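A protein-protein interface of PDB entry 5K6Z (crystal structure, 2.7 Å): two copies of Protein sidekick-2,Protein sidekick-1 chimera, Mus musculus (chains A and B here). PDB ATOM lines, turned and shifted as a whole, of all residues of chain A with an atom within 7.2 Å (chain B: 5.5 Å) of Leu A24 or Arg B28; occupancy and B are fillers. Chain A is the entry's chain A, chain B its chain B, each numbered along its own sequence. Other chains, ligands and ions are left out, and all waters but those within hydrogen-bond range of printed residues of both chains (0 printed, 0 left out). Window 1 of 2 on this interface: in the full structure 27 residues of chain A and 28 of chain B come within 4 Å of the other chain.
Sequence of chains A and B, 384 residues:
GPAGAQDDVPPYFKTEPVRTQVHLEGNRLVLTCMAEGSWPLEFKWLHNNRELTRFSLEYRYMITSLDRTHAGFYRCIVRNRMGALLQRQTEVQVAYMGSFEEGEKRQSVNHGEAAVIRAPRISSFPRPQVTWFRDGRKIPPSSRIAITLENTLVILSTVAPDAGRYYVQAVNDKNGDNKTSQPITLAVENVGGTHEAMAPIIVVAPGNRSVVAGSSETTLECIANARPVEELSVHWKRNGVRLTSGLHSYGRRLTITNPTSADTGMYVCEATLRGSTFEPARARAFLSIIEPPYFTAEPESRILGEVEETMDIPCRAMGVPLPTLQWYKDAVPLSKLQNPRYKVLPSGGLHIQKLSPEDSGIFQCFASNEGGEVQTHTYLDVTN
OD1 of Asn B27 lies within hydrogen-bond range of N of Arg A28, at 2.9 Å. The side-chain amide oxygen (OD1) of Asn A27 sits at hydrogen-bond distance from the backbone NH (N) of Arg B28, at 2.9 Å. The guanidinium group of Arg B28 is in hydrogen-bond range of the backbone carbonyl oxygen of Glu A25. The backbone carbonyl oxygen (O) of Lys A174 sits close to the backbone carbonyl oxygen (O) of Val B30 (3.4 Å).
The backbone carbonyl oxygen (O) of Asn A27 is in hydrogen-bond range of the backbone NH (N) of Leu A66. OD1 of Asn A175 lies close to OD1 of Asn A172, at 3.5 Å. The side-chain amide oxygen (OD1) of Asn A172 is in hydrogen-bond range of the backbone NH (N) of Lys A174 (3.0 Å). The backbone NH (N) of Leu B66 lies within hydrogen-bond range of the backbone carbonyl oxygen (O) of Asn B27 (3.0 Å). OD1 of Asn A175 is in hydrogen-bond range of N of Asp A177 (2.9 Å).
Among the printed residues, merely in contact across the chains: Leu A24 with Arg B28 (3.6 Å), Leu A24 with Val B30 (3.9 Å), Asn A27 with Asn B27 (3.3 Å), Asn A175 with Val B30 (3.2 Å) and Gly A176 with Val B30 (3.9 Å).
Of chain B, only Arg B28 (3.6 Å) and Val B30 (3.9 Å) come within 4 Å of Leu A24. Printed residues of chain B within 4 Å of Asn A27: Asn B27 and Arg B28. Of the printed residues of chain B, Lys A174 touches Val B30. Printed residues of chain B within 4 Å of Asn A175: Val B30. Of the printed residues of chain A, Asn B27 touches Asn A27 (3.3 Å) and Arg A28 (2.9 Å). Arg B28 touches just these residues of chain A: Leu A24 (3.6 Å), Glu A25 (2.6 Å) and Asn A27 (2.9 Å). Of the printed residues of chain A, Val B30 touches Leu A24 (3.9 Å), Lys A174 (3.4 Å), Asn A175 (3.2 Å) and Gly A176 (3.9 Å).
Of the 21 printed residues of chain A, 7 touch a printed residue of chain B. Printed residues of chain A that touch a printed residue of chain B: Leu A24, Glu A25, Asn A27, Arg A28, Lys A174, Asn A175 and Gly A176. Of the 11 printed residues of chain B, 3 touch a printed residue of chain A. Hydrophobic or aromatic side chains of chain B within 4 Å of the printed part of chain A: Val B30. Among the printed residues, 9 pairs touch across the chains.
Asn A27 touches its own counterpart, Asn B27. Asn A27 touches Arg B28, and with the chains exchanged Arg A28 touches Asn B27. Of the 9 pairs that touch across the chains among the printed residues, 3 have their exchanged pair printed and touching as well.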
ATOM      1  N   VAL A  22      18.168  -3.522 -21.121  1.00  0.00           N
ATOM      2  CA  VAL A  22      18.538  -3.491 -22.533  1.00  0.00           C
ATOM      3  C   VAL A  22      17.352  -3.955 -23.366  1.00  0.00           C
ATOM      4  O   VAL A  22      16.769  -5.012 -23.096  1.00  0.00           O
ATOM      5  CB  VAL A  22      19.768  -4.376 -22.804  1.00  0.00           C
ATOM      6  CG1 VAL A  22      20.184  -4.278 -24.266  1.00  0.00           C
ATOM      7  CG2 VAL A  22      20.921  -3.996 -21.885  1.00  0.00           C
ATOM      8  N   HIS A  23      17.005  -3.182 -24.391  1.00  0.00           N
ATOM      9  CA  HIS A  23      15.894  -3.515 -25.267  1.00  0.00           C
ATOM     10  C   HIS A  23      16.352  -3.452 -26.714  1.00  0.00           C
ATOM     11  O   HIS A  23      17.357  -2.817 -27.042  1.00  0.00           O
ATOM     12  CB  HIS A  23      14.704  -2.568 -25.053  1.00  0.00           C
ATOM     13  CG  HIS A  23      14.178  -2.561 -23.651  1.00  0.00           C
ATOM     14  ND1 HIS A  23      13.034  -3.237 -23.283  1.00  0.00           N
ATOM     15  CD2 HIS A  23      14.641  -1.962 -22.528  1.00  0.00           C
ATOM     16  CE1 HIS A  23      12.819  -3.060 -21.991  1.00  0.00           C
ATOM     17  NE2 HIS A  23      13.776  -2.286 -21.512  1.00  0.00           N
ATOM     18  N   LEU A  24      15.594  -4.114 -27.582  1.00  0.00           N
ATOM     19  CA  LEU A  24      15.858  -4.101 -29.014  1.00  0.00           C
ATOM     20  C   LEU A  24      15.029  -3.028 -29.703  1.00  0.00           C
ATOM     21  O   LEU A  24      13.889  -2.758 -29.317  1.00  0.00           O
ATOM     22  CB  LEU A  24      15.537  -5.457 -29.641  1.00  0.00           C
ATOM     23  CG  LEU A  24      16.327  -6.664 -29.162  1.00  0.00           C
ATOM     24  CD1 LEU A  24      15.965  -7.871 -30.012  1.00  0.00           C
ATOM     25  CD2 LEU A  24      17.809  -6.373 -29.224  1.00  0.00           C
ATOM     26  N   GLU A  25      15.608  -2.427 -30.741  1.00  0.00           N
ATOM     27  CA  GLU A  25      14.831  -1.533 -31.587  1.00  0.00           C
ATOM     28  C   GLU A  25      13.634  -2.274 -32.168  1.00  0.00           C
ATOM     29  O   GLU A  25      13.721  -3.454 -32.515  1.00  0.00           O
ATOM     30  CB  GLU A  25      15.695  -0.963 -32.710  1.00  0.00           C
ATOM     31  CG  GLU A  25      16.194   0.445 -32.456  1.00  0.00           C
ATOM     32  CD  GLU A  25      16.878   1.048 -33.663  1.00  0.00           C
ATOM     33  OE1 GLU A  25      17.621   0.321 -34.355  1.00  0.00           O
ATOM     34  OE2 GLU A  25      16.661   2.247 -33.929  1.00  0.00           O
ATOM     35  N   GLY A  26      12.503  -1.583 -32.249  1.00  0.00           N
ATOM     36  CA  GLY A  26      11.291  -2.172 -32.770  1.00  0.00           C
ATOM     37  C   GLY A  26      10.450  -2.919 -31.758  1.00  0.00           C
ATOM     38  O   GLY A  26       9.309  -3.282 -32.075  1.00  0.00           O
ATOM     39  N   ASN A  27      10.972  -3.174 -30.560  1.00  0.00           N
ATOM     40  CA  ASN A  27      10.183  -3.815 -29.523  1.00  0.00           C
ATOM     41  C   ASN A  27       9.379  -2.781 -28.739  1.00  0.00           C
ATOM     42  O   ASN A  27       9.643  -1.574 -28.784  1.00  0.00           O
ATOM     43  CB  ASN A  27      11.079  -4.606 -28.571  1.00  0.00           C
ATOM     44  CG  ASN A  27      11.392  -6.002 -29.079  1.00  0.00           C
ATOM     45  OD1 ASN A  27      10.789  -6.476 -30.042  1.00  0.00           O
ATOM     46  ND2 ASN A  27      12.329  -6.676 -28.415  1.00  0.00           N
ATOM     47  N   ARG A  28       8.388  -3.278 -28.008  1.00  0.00           N
ATOM     48  CA  ARG A  28       7.554  -2.445 -27.154  1.00  0.00           C
ATOM     49  C   ARG A  28       8.188  -2.286 -25.775  1.00  0.00           C
ATOM     50  O   ARG A  28       8.708  -3.246 -25.201  1.00  0.00           O
ATOM     51  CB  ARG A  28       6.163  -3.072 -27.039  1.00  0.00           C
ATOM     52  CG  ARG A  28       5.259  -2.524 -25.964  1.00  0.00           C
ATOM     53  CD  ARG A  28       3.925  -3.271 -25.955  1.00  0.00           C
ATOM     54  NE  ARG A  28       4.002  -4.569 -25.285  1.00  0.00           N
ATOM     55  CZ  ARG A  28       4.234  -5.729 -25.897  1.00  0.00           C
ATOM     56  NH1 ARG A  28       4.420  -5.774 -27.211  1.00  0.00           N
ATOM     57  NH2 ARG A  28       4.280  -6.849 -25.190  1.00  0.00           N
ATOM     58  N   SER A  65       7.265   1.056 -30.376  1.00  0.00           N
ATOM     59  CA  SER A  65       8.384   0.581 -31.180  1.00  0.00           C
ATOM     60  C   SER A  65       9.596   1.439 -30.846  1.00  0.00           C
ATOM     61  O   SER A  65       9.670   2.600 -31.261  1.00  0.00           O
ATOM     62  CB  SER A  65       8.046   0.649 -32.666  1.00  0.00           C
ATOM     63  OG  SER A  65       9.117   0.182 -33.461  1.00  0.00           O
ATOM     64  N   LEU A  66      10.539   0.861 -30.105  1.00  0.00           N
ATOM     65  CA  LEU A  66      11.689   1.606 -29.619  1.00  0.00           C
ATOM     66  C   LEU A  66      12.641   1.980 -30.749  1.00  0.00           C
ATOM     67  O   LEU A  66      12.795   1.257 -31.736  1.00  0.00           O
ATOM     68  CB  LEU A  66      12.440   0.788 -28.573  1.00  0.00           C
ATOM     69  CG  LEU A  66      11.910   0.806 -27.147  1.00  0.00           C
ATOM     70  CD1 LEU A  66      12.429  -0.406 -26.424  1.00  0.00           C
ATOM     71  CD2 LEU A  66      12.360   2.068 -26.443  1.00  0.00           C
ATOM     72  N   ASP A  67      13.300   3.121 -30.573  1.00  0.00           N
ATOM     73  CA  ASP A  67      14.305   3.631 -31.489  1.00  0.00           C
ATOM     74  C   ASP A  67      15.578   3.903 -30.699  1.00  0.00           C
ATOM     75  O   ASP A  67      15.542   4.015 -29.472  1.00  0.00           O
ATOM     76  CB  ASP A  67      13.805   4.909 -32.186  1.00  0.00           C
ATOM     77  CG  ASP A  67      14.751   5.400 -33.261  1.00  0.00           C
ATOM     78  OD1 ASP A  67      14.800   4.771 -34.341  1.00  0.00           O
ATOM     79  OD2 ASP A  67      15.437   6.417 -33.028  1.00  0.00           O
ATOM     80  N   GLN A  93      18.570   1.041 -22.332  1.00  0.00           N
ATOM     81  CA  GLN A  93      19.648   0.902 -23.298  1.00  0.00           C
ATOM     82  C   GLN A  93      19.089   0.182 -24.517  1.00  0.00           C
ATOM     83  O   GLN A  93      18.563  -0.929 -24.398  1.00  0.00           O
ATOM     84  CB  GLN A  93      20.826   0.136 -22.695  1.00  0.00           C
ATOM     85  CG  GLN A  93      21.443   0.803 -21.483  1.00  0.00           C
ATOM     86  CD  GLN A  93      22.482  -0.066 -20.801  1.00  0.00           C
ATOM     87  OE1 GLN A  93      22.282  -1.266 -20.619  1.00  0.00           O
ATOM     88  NE2 GLN A  93      23.600   0.539 -20.418  1.00  0.00           N
ATOM     89  N   VAL A  94      19.193   0.815 -25.678  1.00  0.00           N
ATOM     90  CA  VAL A  94      18.594   0.304 -26.905  1.00  0.00           C
ATOM     91  C   VAL A  94      19.689  -0.309 -27.763  1.00  0.00           C
ATOM     92  O   VAL A  94      20.699   0.344 -28.060  1.00  0.00           O
ATOM     93  CB  VAL A  94      17.849   1.414 -27.662  1.00  0.00           C
ATOM     94  CG1 VAL A  94      17.178   0.850 -28.906  1.00  0.00           C
ATOM     95  CG2 VAL A  94      16.831   2.078 -26.749  1.00  0.00           C
ATOM     96  N   ALA A  95      19.491  -1.561 -28.164  1.00  0.00           N
ATOM     97  CA  ALA A  95      20.480  -2.273 -28.959  1.00  0.00           C
ATOM     98  C   ALA A  95      20.330  -1.895 -30.424  1.00  0.00           C
ATOM     99  O   ALA A  95      19.238  -1.985 -30.992  1.00  0.00           O
ATOM    100  CB  ALA A  95      20.335  -3.781 -28.775  1.00  0.00           C
ATOM    101  N   TYR A  96      21.429  -1.474 -31.033  1.00  0.00           N
ATOM    102  CA  TYR A  96      21.369  -0.958 -32.387  1.00  0.00           C
ATOM    103  C   TYR A  96      22.736  -1.116 -33.032  1.00  0.00           C
ATOM    104  O   TYR A  96      23.765  -1.186 -32.351  1.00  0.00           O
ATOM    105  CB  TYR A  96      20.931   0.511 -32.404  1.00  0.00           C
ATOM    106  CG  TYR A  96      22.020   1.492 -32.020  1.00  0.00           C
ATOM    107  CD1 TYR A  96      22.849   2.052 -32.983  1.00  0.00           C
ATOM    108  CD2 TYR A  96      22.221   1.857 -30.698  1.00  0.00           C
ATOM    109  CE1 TYR A  96      23.845   2.944 -32.643  1.00  0.00           C
ATOM    110  CE2 TYR A  96      23.213   2.755 -30.348  1.00  0.00           C
ATOM    111  CZ  TYR A  96      24.023   3.295 -31.327  1.00  0.00           C
ATOM    112  OH  TYR A  96      25.019   4.188 -30.995  1.00  0.00           O
ATOM    113  N   PHE A 125      25.389  -0.170 -30.027  1.00  0.00           N
ATOM    114  CA  PHE A 125      25.278  -0.629 -28.657  1.00  0.00           C
ATOM    115  C   PHE A 125      24.688  -2.033 -28.617  1.00  0.00           C
ATOM    116  O   PHE A 125      23.647  -2.294 -29.221  1.00  0.00           O
ATOM    117  CB  PHE A 125      24.438   0.298 -27.782  1.00  0.00           C
ATOM    118  CG  PHE A 125      24.313  -0.202 -26.378  1.00  0.00           C
ATOM    119  CD1 PHE A 125      25.304   0.059 -25.452  1.00  0.00           C
ATOM    120  CD2 PHE A 125      23.247  -1.000 -26.002  1.00  0.00           C
ATOM    121  CE1 PHE A 125      25.216  -0.430 -24.169  1.00  0.00           C
ATOM    122  CE2 PHE A 125      23.158  -1.499 -24.720  1.00  0.00           C
ATOM    123  CZ  PHE A 125      24.141  -1.208 -23.802  1.00  0.00           C
ATOM    124  N   ASN A 172      26.453  -7.470 -33.647  1.00  0.00           N
ATOM    125  CA  ASN A 172      25.877  -7.016 -32.390  1.00  0.00           C
ATOM    126  C   ASN A 172      25.259  -8.222 -31.690  1.00  0.00           C
ATOM    127  O   ASN A 172      24.404  -8.905 -32.264  1.00  0.00           O
ATOM    128  CB  ASN A 172      24.839  -5.926 -32.661  1.00  0.00           C
ATOM    129  CG  ASN A 172      24.337  -5.258 -31.398  1.00  0.00           C
ATOM    130  OD1 ASN A 172      23.832  -5.914 -30.482  1.00  0.00           O
ATOM    131  ND2 ASN A 172      24.476  -3.942 -31.343  1.00  0.00           N
ATOM    132  N   ASP A 173      25.699  -8.491 -30.457  1.00  0.00           N
ATOM    133  CA  ASP A 173      25.339  -9.736 -29.788  1.00  0.00           C
ATOM    134  C   ASP A 173      23.950  -9.711 -29.166  1.00  0.00           C
ATOM    135  O   ASP A 173      23.492 -10.755 -28.692  1.00  0.00           O
ATOM    136  CB  ASP A 173      26.374 -10.081 -28.714  1.00  0.00           C
ATOM    137  CG  ASP A 173      26.231  -9.231 -27.468  1.00  0.00           C
ATOM    138  OD1 ASP A 173      25.547  -9.672 -26.521  1.00  0.00           O
ATOM    139  OD2 ASP A 173      26.806  -8.125 -27.429  1.00  0.00           O
ATOM    140  N   LYS A 174      23.266  -8.565 -29.164  1.00  0.00           N
ATOM    141  CA  LYS A 174      21.926  -8.472 -28.595  1.00  0.00           C
ATOM    142  C   LYS A 174      20.818  -8.546 -29.636  1.00  0.00           C
ATOM    143  O   LYS A 174      19.733  -9.056 -29.330  1.00  0.00           O
ATOM    144  CB  LYS A 174      21.764  -7.172 -27.801  1.00  0.00           C
ATOM    145  CG  LYS A 174      22.726  -7.028 -26.644  1.00  0.00           C
ATOM    146  CD  LYS A 174      22.412  -7.996 -25.523  1.00  0.00           C
ATOM    147  CE  LYS A 174      23.447  -7.883 -24.412  1.00  0.00           C
ATOM    148  NZ  LYS A 174      23.044  -8.629 -23.187  1.00  0.00           N
ATOM    149  N   ASN A 175      21.051  -8.035 -30.847  1.00  0.00           N
ATOM    150  CA  ASN A 175      20.067  -8.119 -31.914  1.00  0.00           C
ATOM    151  C   ASN A 175      20.521  -8.959 -33.101  1.00  0.00           C
ATOM    152  O   ASN A 175      19.688  -9.294 -33.949  1.00  0.00           O
ATOM    153  CB  ASN A 175      19.671  -6.712 -32.404  1.00  0.00           C
ATOM    154  CG  ASN A 175      20.824  -5.951 -33.048  1.00  0.00           C
ATOM    155  OD1 ASN A 175      21.893  -6.502 -33.311  1.00  0.00           O
ATOM    156  ND2 ASN A 175      20.596  -4.672 -33.323  1.00  0.00           N
ATOM    157  N   GLY A 176      21.801  -9.309 -33.188  1.00  0.00           N
ATOM    158  CA  GLY A 176      22.282 -10.189 -34.235  1.00  0.00           C
ATOM    159  C   GLY A 176      22.626  -9.524 -35.546  1.00  0.00           C
ATOM    160  O   GLY A 176      22.924 -10.232 -36.516  1.00  0.00           O
ATOM    161  N   ASP A 177      22.591  -8.195 -35.614  1.00  0.00           N
ATOM    162  CA  ASP A 177      22.931  -7.496 -36.844  1.00  0.00           C
ATOM    163  C   ASP A 177      24.385  -7.741 -37.207  1.00  0.00           C
ATOM    164  O   ASP A 177      25.254  -7.808 -36.333  1.00  0.00           O
ATOM    165  CB  ASP A 177      22.694  -5.995 -36.695  1.00  0.00           C
ATOM    166  CG  ASP A 177      21.272  -5.600 -36.981  1.00  0.00           C
ATOM    167  OD1 ASP A 177      20.395  -6.487 -36.945  1.00  0.00           O
ATOM    168  OD2 ASP A 177      21.030  -4.402 -37.239  1.00  0.00           O
ATOM    169  N   HIS B  23      11.666 -10.583 -21.053  1.00  0.00           N
ATOM    170  CA  HIS B  23      11.156 -10.052 -22.307  1.00  0.00           C
ATOM    171  C   HIS B  23       9.637 -10.052 -22.256  1.00  0.00           C
ATOM    172  O   HIS B  23       9.021 -10.807 -21.500  1.00  0.00           O
ATOM    173  CB  HIS B  23      11.641 -10.866 -23.511  1.00  0.00           C
ATOM    174  CG  HIS B  23      13.131 -10.941 -23.637  1.00  0.00           C
ATOM    175  ND1 HIS B  23      13.831 -10.266 -24.614  1.00  0.00           N
ATOM    176  CD2 HIS B  23      14.054 -11.624 -22.918  1.00  0.00           C
ATOM    177  CE1 HIS B  23      15.120 -10.523 -24.487  1.00  0.00           C
ATOM    178  NE2 HIS B  23      15.282 -11.344 -23.465  1.00  0.00           N
ATOM    179  N   GLY B  26       5.038 -10.952 -27.241  1.00  0.00           N
ATOM    180  CA  GLY B  26       4.828 -10.185 -28.450  1.00  0.00           C
ATOM    181  C   GLY B  26       6.045  -9.447 -28.968  1.00  0.00           C
ATOM    182  O   GLY B  26       5.993  -8.906 -30.079  1.00  0.00           O
ATOM    183  N   ASN B  27       7.130  -9.403 -28.202  1.00  0.00           N
ATOM    184  CA  ASN B  27       8.372  -8.784 -28.636  1.00  0.00           C
ATOM    185  C   ASN B  27       9.282  -9.805 -29.316  1.00  0.00           C
ATOM    186  O   ASN B  27       9.104 -11.021 -29.197  1.00  0.00           O
ATOM    187  CB  ASN B  27       9.104  -8.151 -27.450  1.00  0.00           C
ATOM    188  CG  ASN B  27       8.715  -6.708 -27.222  1.00  0.00           C
ATOM    189  OD1 ASN B  27       7.860  -6.165 -27.916  1.00  0.00           O
ATOM    190  ND2 ASN B  27       9.340  -6.079 -26.236  1.00  0.00           N
ATOM    191  N   ARG B  28      10.278  -9.285 -30.026  1.00  0.00           N
ATOM    192  CA  ARG B  28      11.244 -10.104 -30.741  1.00  0.00           C
ATOM    193  C   ARG B  28      12.385 -10.497 -29.810  1.00  0.00           C
ATOM    194  O   ARG B  28      12.927  -9.652 -29.089  1.00  0.00           O
ATOM    195  CB  ARG B  28      11.777  -9.341 -31.953  1.00  0.00           C
ATOM    196  CG  ARG B  28      12.878 -10.035 -32.731  1.00  0.00           C
ATOM    197  CD  ARG B  28      13.239  -9.206 -33.952  1.00  0.00           C
ATOM    198  NE  ARG B  28      13.330  -7.791 -33.608  1.00  0.00           N
ATOM    199  CZ  ARG B  28      14.442  -7.067 -33.683  1.00  0.00           C
ATOM    200  NH1 ARG B  28      15.571  -7.619 -34.112  1.00  0.00           N
ATOM    201  NH2 ARG B  28      14.421  -5.785 -33.338  1.00  0.00           N
ATOM    202  N   LEU B  29      12.735 -11.781 -29.819  1.00  0.00           N
ATOM    203  CA  LEU B  29      13.910 -12.291 -29.127  1.00  0.00           C
ATOM    204  C   LEU B  29      14.977 -12.623 -30.162  1.00  0.00           C
ATOM    205  O   LEU B  29      14.678 -13.227 -31.199  1.00  0.00           O
ATOM    206  CB  LEU B  29      13.568 -13.532 -28.295  1.00  0.00           C
ATOM    207  CG  LEU B  29      14.700 -14.237 -27.532  1.00  0.00           C
ATOM    208  CD1 LEU B  29      15.141 -13.421 -26.328  1.00  0.00           C
ATOM    209  CD2 LEU B  29      14.286 -15.631 -27.099  1.00  0.00           C
ATOM    210  N   VAL B  30      16.213 -12.208 -29.893  1.00  0.00           N
ATOM    211  CA  VAL B  30      17.361 -12.606 -30.696  1.00  0.00           C
ATOM    212  C   VAL B  30      18.427 -13.118 -29.749  1.00  0.00           C
ATOM    213  O   VAL B  30      18.940 -12.359 -28.920  1.00  0.00           O
ATOM    214  CB  VAL B  30      17.924 -11.462 -31.555  1.00  0.00           C
ATOM    215  CG1 VAL B  30      19.037 -11.999 -32.454  1.00  0.00           C
ATOM    216  CG2 VAL B  30      16.830 -10.802 -32.380  1.00  0.00           C
ATOM    217  N   MET B  62      16.162 -16.558 -33.468  1.00  0.00           N
ATOM    218  CA  MET B  62      15.220 -15.449 -33.416  1.00  0.00           C
ATOM    219  C   MET B  62      13.793 -15.954 -33.269  1.00  0.00           C
ATOM    220  O   MET B  62      13.369 -16.863 -33.991  1.00  0.00           O
ATOM    221  CB  MET B  62      15.326 -14.561 -34.660  1.00  0.00           C
ATOM    222  CG  MET B  62      14.592 -13.231 -34.488  1.00  0.00           C
ATOM    223  SD  MET B  62      14.626 -12.143 -35.925  1.00  0.00           S
ATOM    224  CE  MET B  62      13.312 -12.845 -36.923  1.00  0.00           C
ATOM    225  N   ILE B  63      13.060 -15.352 -32.334  1.00  0.00           N
ATOM    226  CA  ILE B  63      11.619 -15.530 -32.189  1.00  0.00           C
ATOM    227  C   ILE B  63      10.971 -14.186 -32.489  1.00  0.00           C
ATOM    228  O   ILE B  63      11.207 -13.204 -31.773  1.00  0.00           O
ATOM    229  CB  ILE B  63      11.244 -16.017 -30.781  1.00  0.00           C
ATOM    230  CG1 ILE B  63      12.093 -17.223 -30.384  1.00  0.00           C
ATOM    231  CG2 ILE B  63       9.771 -16.368 -30.717  1.00  0.00           C
ATOM    232  CD1 ILE B  63      11.813 -17.715 -28.985  1.00  0.00           C
ATOM    233  N   THR B  64      10.160 -14.136 -33.547  1.00  0.00           N
ATOM    234  CA  THR B  64       9.581 -12.862 -33.973  1.00  0.00           C
ATOM    235  C   THR B  64       8.606 -12.313 -32.940  1.00  0.00           C
ATOM    236  O   THR B  64       8.640 -11.118 -32.623  1.00  0.00           O
ATOM    237  CB  THR B  64       8.887 -13.022 -35.326  1.00  0.00           C
ATOM    238  OG1 THR B  64       9.820 -13.541 -36.279  1.00  0.00           O
ATOM    239  CG2 THR B  64       8.372 -11.680 -35.818  1.00  0.00           C
ATOM    240  N   SER B  65       7.729 -13.160 -32.404  1.00  0.00           N
ATOM    241  CA  SER B  65       6.759 -12.738 -31.395  1.00  0.00           C
ATOM    242  C   SER B  65       6.734 -13.773 -30.280  1.00  0.00           C
ATOM    243  O   SER B  65       6.277 -14.903 -30.489  1.00  0.00           O
ATOM    244  CB  SER B  65       5.369 -12.559 -31.999  1.00  0.00           C
ATOM    245  OG  SER B  65       4.433 -12.221 -30.991  1.00  0.00           O
ATOM    246  N   LEU B  66       7.203 -13.379 -29.098  1.00  0.00           N
ATOM    247  CA  LEU B  66       7.323 -14.294 -27.973  1.00  0.00           C
ATOM    248  C   LEU B  66       5.965 -14.693 -27.411  1.00  0.00           C
ATOM    249  O   LEU B  66       5.008 -13.915 -27.404  1.00  0.00           O
ATOM    250  CB  LEU B  66       8.155 -13.662 -26.861  1.00  0.00           C
ATOM    251  CG  LEU B  66       9.661 -13.711 -27.064  1.00  0.00           C
ATOM    252  CD1 LEU B  66      10.322 -12.845 -26.029  1.00  0.00           C
ATOM    253  CD2 LEU B  66      10.146 -15.138 -26.959  1.00  0.00           C
